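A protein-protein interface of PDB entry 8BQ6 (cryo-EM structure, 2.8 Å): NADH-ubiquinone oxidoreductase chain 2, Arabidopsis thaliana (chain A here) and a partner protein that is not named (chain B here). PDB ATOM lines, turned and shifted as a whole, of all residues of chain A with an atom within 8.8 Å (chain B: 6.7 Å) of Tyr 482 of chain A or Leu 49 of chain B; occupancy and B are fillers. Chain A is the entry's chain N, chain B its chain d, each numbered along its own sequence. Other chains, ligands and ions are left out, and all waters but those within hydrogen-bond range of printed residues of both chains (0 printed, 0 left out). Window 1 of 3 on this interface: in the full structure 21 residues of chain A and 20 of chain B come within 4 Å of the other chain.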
ATOM      1  N   PHE A 475     -19.031 -20.008   6.744  1.00  0.00           N
ATOM      2  CA  PHE A 475     -18.699 -18.719   7.341  1.00  0.00           C
ATOM      3  C   PHE A 475     -19.947 -17.855   7.497  1.00  0.00           C
ATOM      4  O   PHE A 475     -20.165 -17.243   8.547  1.00  0.00           O
ATOM      5  CB  PHE A 475     -17.645 -17.993   6.502  1.00  0.00           C
ATOM      6  CG  PHE A 475     -17.289 -16.629   7.028  1.00  0.00           C
ATOM      7  CD1 PHE A 475     -18.035 -15.517   6.672  1.00  0.00           C
ATOM      8  CD2 PHE A 475     -16.208 -16.457   7.873  1.00  0.00           C
ATOM      9  CE1 PHE A 475     -17.722 -14.267   7.159  1.00  0.00           C
ATOM     10  CE2 PHE A 475     -15.885 -15.204   8.355  1.00  0.00           C
ATOM     11  CZ  PHE A 475     -16.644 -14.109   7.998  1.00  0.00           C
ATOM     12  N   THR A 477     -23.132 -18.615   7.749  1.00  0.00           N
ATOM     13  CA  THR A 477     -24.091 -19.044   8.762  1.00  0.00           C
ATOM     14  C   THR A 477     -23.531 -18.977  10.178  1.00  0.00           C
ATOM     15  O   THR A 477     -24.297 -18.801  11.130  1.00  0.00           O
ATOM     16  CB  THR A 477     -24.563 -20.470   8.485  1.00  0.00           C
ATOM     17  OG1 THR A 477     -23.448 -21.364   8.572  1.00  0.00           O
ATOM     18  CG2 THR A 477     -25.169 -20.568   7.108  1.00  0.00           C
ATOM     19  N   LEU A 478     -22.217 -19.117  10.346  1.00  0.00           N
ATOM     20  CA  LEU A 478     -21.641 -19.369  11.659  1.00  0.00           C
ATOM     21  C   LEU A 478     -20.670 -18.299  12.135  1.00  0.00           C
ATOM     22  O   LEU A 478     -20.108 -18.446  13.225  1.00  0.00           O
ATOM     23  CB  LEU A 478     -20.928 -20.724  11.663  1.00  0.00           C
ATOM     24  CG  LEU A 478     -21.786 -21.944  11.346  1.00  0.00           C
ATOM     25  CD1 LEU A 478     -20.899 -23.143  11.110  1.00  0.00           C
ATOM     26  CD2 LEU A 478     -22.754 -22.210  12.479  1.00  0.00           C
ATOM     27  N   PHE A 479     -20.506 -17.193  11.410  1.00  0.00           N
ATOM     28  CA  PHE A 479     -19.490 -16.186  11.829  1.00  0.00           C
ATOM     29  C   PHE A 479     -19.901 -15.552  13.163  1.00  0.00           C
ATOM     30  O   PHE A 479     -19.017 -15.358  14.010  1.00  0.00           O
ATOM     31  CB  PHE A 479     -19.299 -15.111  10.753  1.00  0.00           C
ATOM     32  CG  PHE A 479     -18.709 -13.802  11.214  1.00  0.00           C
ATOM     33  CD1 PHE A 479     -17.359 -13.695  11.509  1.00  0.00           C
ATOM     34  CD2 PHE A 479     -19.501 -12.673  11.342  1.00  0.00           C
ATOM     35  CE1 PHE A 479     -16.818 -12.492  11.927  1.00  0.00           C
ATOM     36  CE2 PHE A 479     -18.959 -11.471  11.769  1.00  0.00           C
ATOM     37  CZ  PHE A 479     -17.619 -11.382  12.058  1.00  0.00           C
ATOM     38  N   LEU A 480     -21.191 -15.248  13.341  1.00  0.00           N
ATOM     39  CA  LEU A 480     -21.637 -14.528  14.566  1.00  0.00           C
ATOM     40  C   LEU A 480     -21.435 -15.394  15.813  1.00  0.00           C
ATOM     41  O   LEU A 480     -21.608 -14.850  16.910  1.00  0.00           O
ATOM     42  CB  LEU A 480     -23.099 -14.099  14.399  1.00  0.00           C
ATOM     43  CG  LEU A 480     -23.298 -12.799  13.618  1.00  0.00           C
ATOM     44  CD1 LEU A 480     -24.663 -12.196  13.900  1.00  0.00           C
ATOM     45  CD2 LEU A 480     -22.203 -11.797  13.945  1.00  0.00           C
ATOM     46  N   LEU A 481     -21.074 -16.672  15.662  1.00  0.00           N
ATOM     47  CA  LEU A 481     -20.767 -17.494  16.826  1.00  0.00           C
ATOM     48  C   LEU A 481     -19.352 -17.249  17.336  1.00  0.00           C
ATOM     49  O   LEU A 481     -19.101 -17.377  18.540  1.00  0.00           O
ATOM     50  CB  LEU A 481     -20.945 -18.972  16.482  1.00  0.00           C
ATOM     51  CG  LEU A 481     -22.361 -19.468  16.183  1.00  0.00           C
ATOM     52  CD1 LEU A 481     -22.350 -20.951  15.855  1.00  0.00           C
ATOM     53  CD2 LEU A 481     -23.296 -19.189  17.337  1.00  0.00           C
ATOM     54  N   TYR A 482     -18.410 -16.933  16.444  1.00  0.00           N
ATOM     55  CA  TYR A 482     -17.011 -16.720  16.824  1.00  0.00           C
ATOM     56  C   TYR A 482     -16.424 -15.541  16.052  1.00  0.00           C
ATOM     57  O   TYR A 482     -15.501 -15.702  15.250  1.00  0.00           O
ATOM     58  CB  TYR A 482     -16.200 -17.991  16.582  1.00  0.00           C
ATOM     59  CG  TYR A 482     -14.910 -18.043  17.356  1.00  0.00           C
ATOM     60  CD1 TYR A 482     -14.908 -17.984  18.742  1.00  0.00           C
ATOM     61  CD2 TYR A 482     -13.693 -18.154  16.704  1.00  0.00           C
ATOM     62  CE1 TYR A 482     -13.728 -18.031  19.456  1.00  0.00           C
ATOM     63  CE2 TYR A 482     -12.509 -18.201  17.409  1.00  0.00           C
ATOM     64  CZ  TYR A 482     -12.533 -18.141  18.785  1.00  0.00           C
ATOM     65  OH  TYR A 482     -11.355 -18.189  19.492  1.00  0.00           O
ATOM     66  N   PRO A 483     -16.918 -14.328  16.297  1.00  0.00           N
ATOM     67  CA  PRO A 483     -16.464 -13.161  15.527  1.00  0.00           C
ATOM     68  C   PRO A 483     -15.256 -12.440  16.106  1.00  0.00           C
ATOM     69  O   PRO A 483     -14.874 -11.397  15.567  1.00  0.00           O
ATOM     70  CB  PRO A 483     -17.694 -12.253  15.586  1.00  0.00           C
ATOM     71  CG  PRO A 483     -18.209 -12.492  16.949  1.00  0.00           C
ATOM     72  CD  PRO A 483     -17.982 -13.957  17.246  1.00  0.00           C
ATOM     73  N   SER A 484     -14.663 -12.971  17.174  1.00  0.00           N
ATOM     74  CA  SER A 484     -13.583 -12.277  17.872  1.00  0.00           C
ATOM     75  C   SER A 484     -12.379 -11.955  16.996  1.00  0.00           C
ATOM     76  O   SER A 484     -11.882 -10.816  17.073  1.00  0.00           O
ATOM     77  CB  SER A 484     -13.170 -13.104  19.094  1.00  0.00           C
ATOM     78  OG  SER A 484     -11.973 -12.613  19.667  1.00  0.00           O
ATOM     79  N   PRO A 485     -11.836 -12.879  16.185  1.00  0.00           N
ATOM     80  CA  PRO A 485     -10.628 -12.527  15.420  1.00  0.00           C
ATOM     81  C   PRO A 485     -10.823 -11.360  14.468  1.00  0.00           C
ATOM     82  O   PRO A 485      -9.952 -10.486  14.401  1.00  0.00           O
ATOM     83  CB  PRO A 485     -10.293 -13.823  14.666  1.00  0.00           C
ATOM     84  CG  PRO A 485     -11.009 -14.889  15.380  1.00  0.00           C
ATOM     85  CD  PRO A 485     -12.239 -14.274  15.941  1.00  0.00           C
ATOM     86  N   LEU A 486     -11.937 -11.312  13.734  1.00  0.00           N
ATOM     87  CA  LEU A 486     -12.149 -10.200  12.813  1.00  0.00           C
ATOM     88  C   LEU A 486     -12.274  -8.881  13.565  1.00  0.00           C
ATOM     89  O   LEU A 486     -11.727  -7.859  13.135  1.00  0.00           O
ATOM     90  CB  LEU A 486     -13.390 -10.439  11.952  1.00  0.00           C
ATOM     91  CG  LEU A 486     -13.625  -9.449  10.802  1.00  0.00           C
ATOM     92  CD1 LEU A 486     -12.429  -9.370   9.847  1.00  0.00           C
ATOM     93  CD2 LEU A 486     -14.917  -9.746  10.055  1.00  0.00           C
ATOM     94  N   PHE A 487     -12.988  -8.885  14.691  1.00  0.00           N
ATOM     95  CA  PHE A 487     -13.144  -7.663  15.477  1.00  0.00           C
ATOM     96  C   PHE A 487     -11.801  -7.170  15.980  1.00  0.00           C
ATOM     97  O   PHE A 487     -11.470  -5.981  15.862  1.00  0.00           O
ATOM     98  CB  PHE A 487     -14.088  -7.914  16.646  1.00  0.00           C
ATOM     99  CG  PHE A 487     -15.490  -8.180  16.233  1.00  0.00           C
ATOM    100  CD1 PHE A 487     -15.896  -7.942  14.932  1.00  0.00           C
ATOM    101  CD2 PHE A 487     -16.403  -8.684  17.132  1.00  0.00           C
ATOM    102  CE1 PHE A 487     -17.187  -8.187  14.545  1.00  0.00           C
ATOM    103  CE2 PHE A 487     -17.694  -8.932  16.747  1.00  0.00           C
ATOM    104  CZ  PHE A 487     -18.088  -8.682  15.452  1.00  0.00           C
ATOM    105  N   VAL B  44      -6.732 -28.616  12.255  1.00  0.00           N
ATOM    106  CA  VAL B  44      -5.562 -27.744  12.259  1.00  0.00           C
ATOM    107  C   VAL B  44      -5.988 -26.285  12.153  1.00  0.00           C
ATOM    108  O   VAL B  44      -5.494 -25.416  12.885  1.00  0.00           O
ATOM    109  CB  VAL B  44      -4.602 -28.151  11.126  1.00  0.00           C
ATOM    110  CG1 VAL B  44      -3.737 -26.987  10.698  1.00  0.00           C
ATOM    111  CG2 VAL B  44      -3.742 -29.313  11.572  1.00  0.00           C
ATOM    112  N   PHE B  45      -6.931 -25.999  11.255  1.00  0.00           N
ATOM    113  CA  PHE B  45      -7.379 -24.627  11.054  1.00  0.00           C
ATOM    114  C   PHE B  45      -8.066 -24.068  12.298  1.00  0.00           C
ATOM    115  O   PHE B  45      -7.849 -22.906  12.658  1.00  0.00           O
ATOM    116  CB  PHE B  45      -8.294 -24.574   9.832  1.00  0.00           C
ATOM    117  CG  PHE B  45      -9.122 -23.334   9.738  1.00  0.00           C
ATOM    118  CD1 PHE B  45     -10.425 -23.322  10.201  1.00  0.00           C
ATOM    119  CD2 PHE B  45      -8.612 -22.189   9.155  1.00  0.00           C
ATOM    120  CE1 PHE B  45     -11.193 -22.187  10.109  1.00  0.00           C
ATOM    121  CE2 PHE B  45      -9.377 -21.050   9.057  1.00  0.00           C
ATOM    122  CZ  PHE B  45     -10.672 -21.047   9.537  1.00  0.00           C
ATOM    123  N   ALA B  46      -8.893 -24.871  12.976  1.00  0.00           N
ATOM    124  CA  ALA B  46      -9.560 -24.365  14.174  1.00  0.00           C
ATOM    125  C   ALA B  46      -8.563 -24.083  15.296  1.00  0.00           C
ATOM    126  O   ALA B  46      -8.641 -23.035  15.960  1.00  0.00           O
ATOM    127  CB  ALA B  46     -10.635 -25.347  14.639  1.00  0.00           C
ATOM    128  N   ASN B  47      -7.607 -24.992  15.518  1.00  0.00           N
ATOM    129  CA  ASN B  47      -6.621 -24.739  16.566  1.00  0.00           C
ATOM    130  C   ASN B  47      -5.786 -23.501  16.254  1.00  0.00           C
ATOM    131  O   ASN B  47      -5.523 -22.672  17.141  1.00  0.00           O
ATOM    132  CB  ASN B  47      -5.724 -25.957  16.762  1.00  0.00           C
ATOM    133  CG  ASN B  47      -6.133 -26.786  17.958  1.00  0.00           C
ATOM    134  OD1 ASN B  47      -7.177 -27.435  17.951  1.00  0.00           O
ATOM    135  ND2 ASN B  47      -5.317 -26.753  19.003  1.00  0.00           N
ATOM    136  N   GLN B  48      -5.370 -23.352  14.995  1.00  0.00           N
ATOM    137  CA  GLN B  48      -4.562 -22.198  14.625  1.00  0.00           C
ATOM    138  C   GLN B  48      -5.360 -20.909  14.744  1.00  0.00           C
ATOM    139  O   GLN B  48      -4.813 -19.870  15.122  1.00  0.00           O
ATOM    140  CB  GLN B  48      -4.021 -22.376  13.211  1.00  0.00           C
ATOM    141  CG  GLN B  48      -2.929 -23.426  13.100  1.00  0.00           C
ATOM    142  CD  GLN B  48      -1.811 -23.228  14.104  1.00  0.00           C
ATOM    143  OE1 GLN B  48      -0.858 -22.497  13.845  1.00  0.00           O
ATOM    144  NE2 GLN B  48      -1.915 -23.887  15.252  1.00  0.00           N
ATOM    145  N   LEU B  49      -6.657 -20.951  14.430  1.00  0.00           N
ATOM    146  CA  LEU B  49      -7.479 -19.761  14.608  1.00  0.00           C
ATOM    147  C   LEU B  49      -7.549 -19.362  16.072  1.00  0.00           C
ATOM    148  O   LEU B  49      -7.492 -18.171  16.401  1.00  0.00           O
ATOM    149  CB  LEU B  49      -8.881 -19.989  14.050  1.00  0.00           C
ATOM    150  CG  LEU B  49      -9.778 -18.752  14.099  1.00  0.00           C
ATOM    151  CD1 LEU B  49      -9.388 -17.765  13.012  1.00  0.00           C
ATOM    152  CD2 LEU B  49     -11.234 -19.143  13.961  1.00  0.00           C
ATOM    153  N   VAL B  50      -7.676 -20.340  16.968  1.00  0.00           N
ATOM    154  CA  VAL B  50      -7.721 -20.020  18.395  1.00  0.00           C
ATOM    155  C   VAL B  50      -6.409 -19.371  18.841  1.00  0.00           C
ATOM    156  O   VAL B  50      -6.402 -18.334  19.527  1.00  0.00           O
ATOM    157  CB  VAL B  50      -8.057 -21.281  19.211  1.00  0.00           C
ATOM    158  CG1 VAL B  50      -7.689 -21.095  20.665  1.00  0.00           C
ATOM    159  CG2 VAL B  50      -9.538 -21.598  19.075  1.00  0.00           C
ATOM    160  N   LYS B  51      -5.276 -19.949  18.428  1.00  0.00           N
ATOM    161  CA  LYS B  51      -3.986 -19.352  18.775  1.00  0.00           C
ATOM    162  C   LYS B  51      -3.844 -17.946  18.195  1.00  0.00           C
ATOM    163  O   LYS B  51      -3.345 -17.026  18.865  1.00  0.00           O
ATOM    164  CB  LYS B  51      -2.843 -20.243  18.296  1.00  0.00           C
ATOM    165  CG  LYS B  51      -2.624 -21.469  19.154  1.00  0.00           C
ATOM    166  CD  LYS B  51      -2.582 -22.724  18.307  1.00  0.00           C
ATOM    167  CE  LYS B  51      -2.001 -23.893  19.080  1.00  0.00           C
ATOM    168  NZ  LYS B  51      -0.564 -23.682  19.387  1.00  0.00           N
ATOM    169  N   TRP B  52      -4.279 -17.760  16.950  1.00  0.00           N
ATOM    170  CA  TRP B  52      -4.174 -16.456  16.315  1.00  0.00           C
ATOM    171  C   TRP B  52      -5.027 -15.424  17.033  1.00  0.00           C
ATOM    172  O   TRP B  52      -4.619 -14.269  17.177  1.00  0.00           O
ATOM    173  CB  TRP B  52      -4.576 -16.550  14.847  1.00  0.00           C
ATOM    174  CG  TRP B  52      -4.379 -15.270  14.129  1.00  0.00           C
ATOM    175  CD1 TRP B  52      -3.250 -14.513  14.107  1.00  0.00           C
ATOM    176  CD2 TRP B  52      -5.346 -14.574  13.339  1.00  0.00           C
ATOM    177  NE1 TRP B  52      -3.446 -13.390  13.347  1.00  0.00           N
ATOM    178  CE2 TRP B  52      -4.726 -13.404  12.861  1.00  0.00           C
ATOM    179  CE3 TRP B  52      -6.672 -14.828  12.985  1.00  0.00           C
ATOM    180  CZ2 TRP B  52      -5.388 -12.490  12.050  1.00  0.00           C
ATOM    181  CZ3 TRP B  52      -7.326 -13.920  12.179  1.00  0.00           C
ATOM    182  CH2 TRP B  52      -6.685 -12.767  11.721  1.00  0.00           C
ATOM    183  N   ASP B  53      -6.222 -15.819  17.472  1.00  0.00           N
ATOM    184  CA  ASP B  53      -7.072 -14.913  18.236  1.00  0.00           C
ATOM    185  C   ASP B  53      -6.399 -14.486  19.534  1.00  0.00           C
ATOM    186  O   ASP B  53      -6.441 -13.304  19.909  1.00  0.00           O
ATOM    187  CB  ASP B  53      -8.413 -15.590  18.511  1.00  0.00           C
ATOM    188  CG  ASP B  53      -9.453 -14.635  19.041  1.00  0.00           C
ATOM    189  OD1 ASP B  53      -9.464 -13.465  18.607  1.00  0.00           O
ATOM    190  OD2 ASP B  53     -10.278 -15.062  19.873  1.00  0.00           O
ATOM    191  N   VAL B  54      -5.768 -15.433  20.233  1.00  0.00           N
ATOM    192  CA  VAL B  54      -5.068 -15.075  21.467  1.00  0.00           C
ATOM    193  C   VAL B  54      -3.979 -14.046  21.179  1.00  0.00           C
ATOM    194  O   VAL B  54      -3.866 -13.014  21.861  1.00  0.00           O
ATOM    195  CB  VAL B  54      -4.497 -16.333  22.141  1.00  0.00           C
ATOM    196  CG1 VAL B  54      -3.815 -15.969  23.439  1.00  0.00           C
ATOM    197  CG2 VAL B  54      -5.612 -17.325  22.404  1.00  0.00           C
ATOM    198  N   LYS B  57      -5.327 -10.533  20.425  1.00  0.00           N
ATOM    199  CA  LYS B  57      -5.742  -9.815  21.661  1.00  0.00           C
ATOM    200  C   LYS B  57      -4.527  -9.132  22.298  1.00  0.00           C
ATOM    201  O   LYS B  57      -4.639  -7.936  22.603  1.00  0.00           O
ATOM    202  CB  LYS B  57      -6.415 -10.781  22.639  1.00  0.00           C
ATOM    203  CG  LYS B  57      -7.754 -11.338  22.174  1.00  0.00           C
ATOM    204  CD  LYS B  57      -8.378 -12.307  23.154  1.00  0.00           C
ATOM    205  CE  LYS B  57      -9.720 -12.831  22.688  1.00  0.00           C
ATOM    206  NZ  LYS B  57     -10.299 -13.795  23.652  1.00  0.00           N
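Of the printed residues of chain B, Tyr 482 of chain A touches Leu 49, Val 50 and Asp 53.
Of the printed residues of chain B, Pro 485 of chain A touches Trp 52 and Asp 53.
Of the printed residues of chain A, Asp 53 of chain B touches Tyr 482, Ser 484 and Pro 485.
Of the printed residues of chain A, Val 50 of chain B touches Tyr 482 (3.9 Å).
Phe 475 of chain A touches none of the printed residues of chain B.
Phe 45 of chain B touches none of the printed residues of chain A.
The nearest printed residue of chain B that does not touch Ser 484 of chain A is Val 54 of chain B (6.8 Å).
Of the 12 printed residues of chain B, 5 touch a printed residue of chain A.
Printed residues of chain B that touch a printed residue of chain A: Leu 49, Val 50, Trp 52, Asp 53 and Lys 57.
Hydrophobic or aromatic side chains of chain B within 4 Å of the printed part of chain A: Leu 49, Val 50 and Trp 52.
Printed residues of chain A that touch a printed residue of chain B: Tyr 482, Ser 484 and Pro 485.
Hydrophobic or aromatic side chains of chain A within 4 Å of the printed part of chain B: Tyr 482 and Pro 485.
The side-chain carboxylate (OD2) of Asp 53 of chain B lies within salt-bridge range of the side-chain amino group (NZ) of Lys 57 of chain B (3.99 Å).
Among the printed residues, pairs that only touch across the chains: Ser 484 of chain A with Lys 57 of chain B (3.8 Å), Tyr 482 of chain A with Leu 49 of chain B (3.8 Å), Pro 485 of chain A with Trp 52 of chain B (3.9 Å) and Tyr 482 of chain A with Val 50 of chain B (3.9 Å).
The side-chain hydroxyl (OH) of Tyr 482 of chain A sits at hydrogen-bond distance from the side-chain carboxylate (OD2) of Asp 53 of chain B (3.3 Å).
OD1 of Asp 53 of chain B is in hydrogen-bond range of OG of Ser 484 of chain A (2.9 Å).
N of Pro 485 of chain A lies close to OD1 of Asp 53 of chain B.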
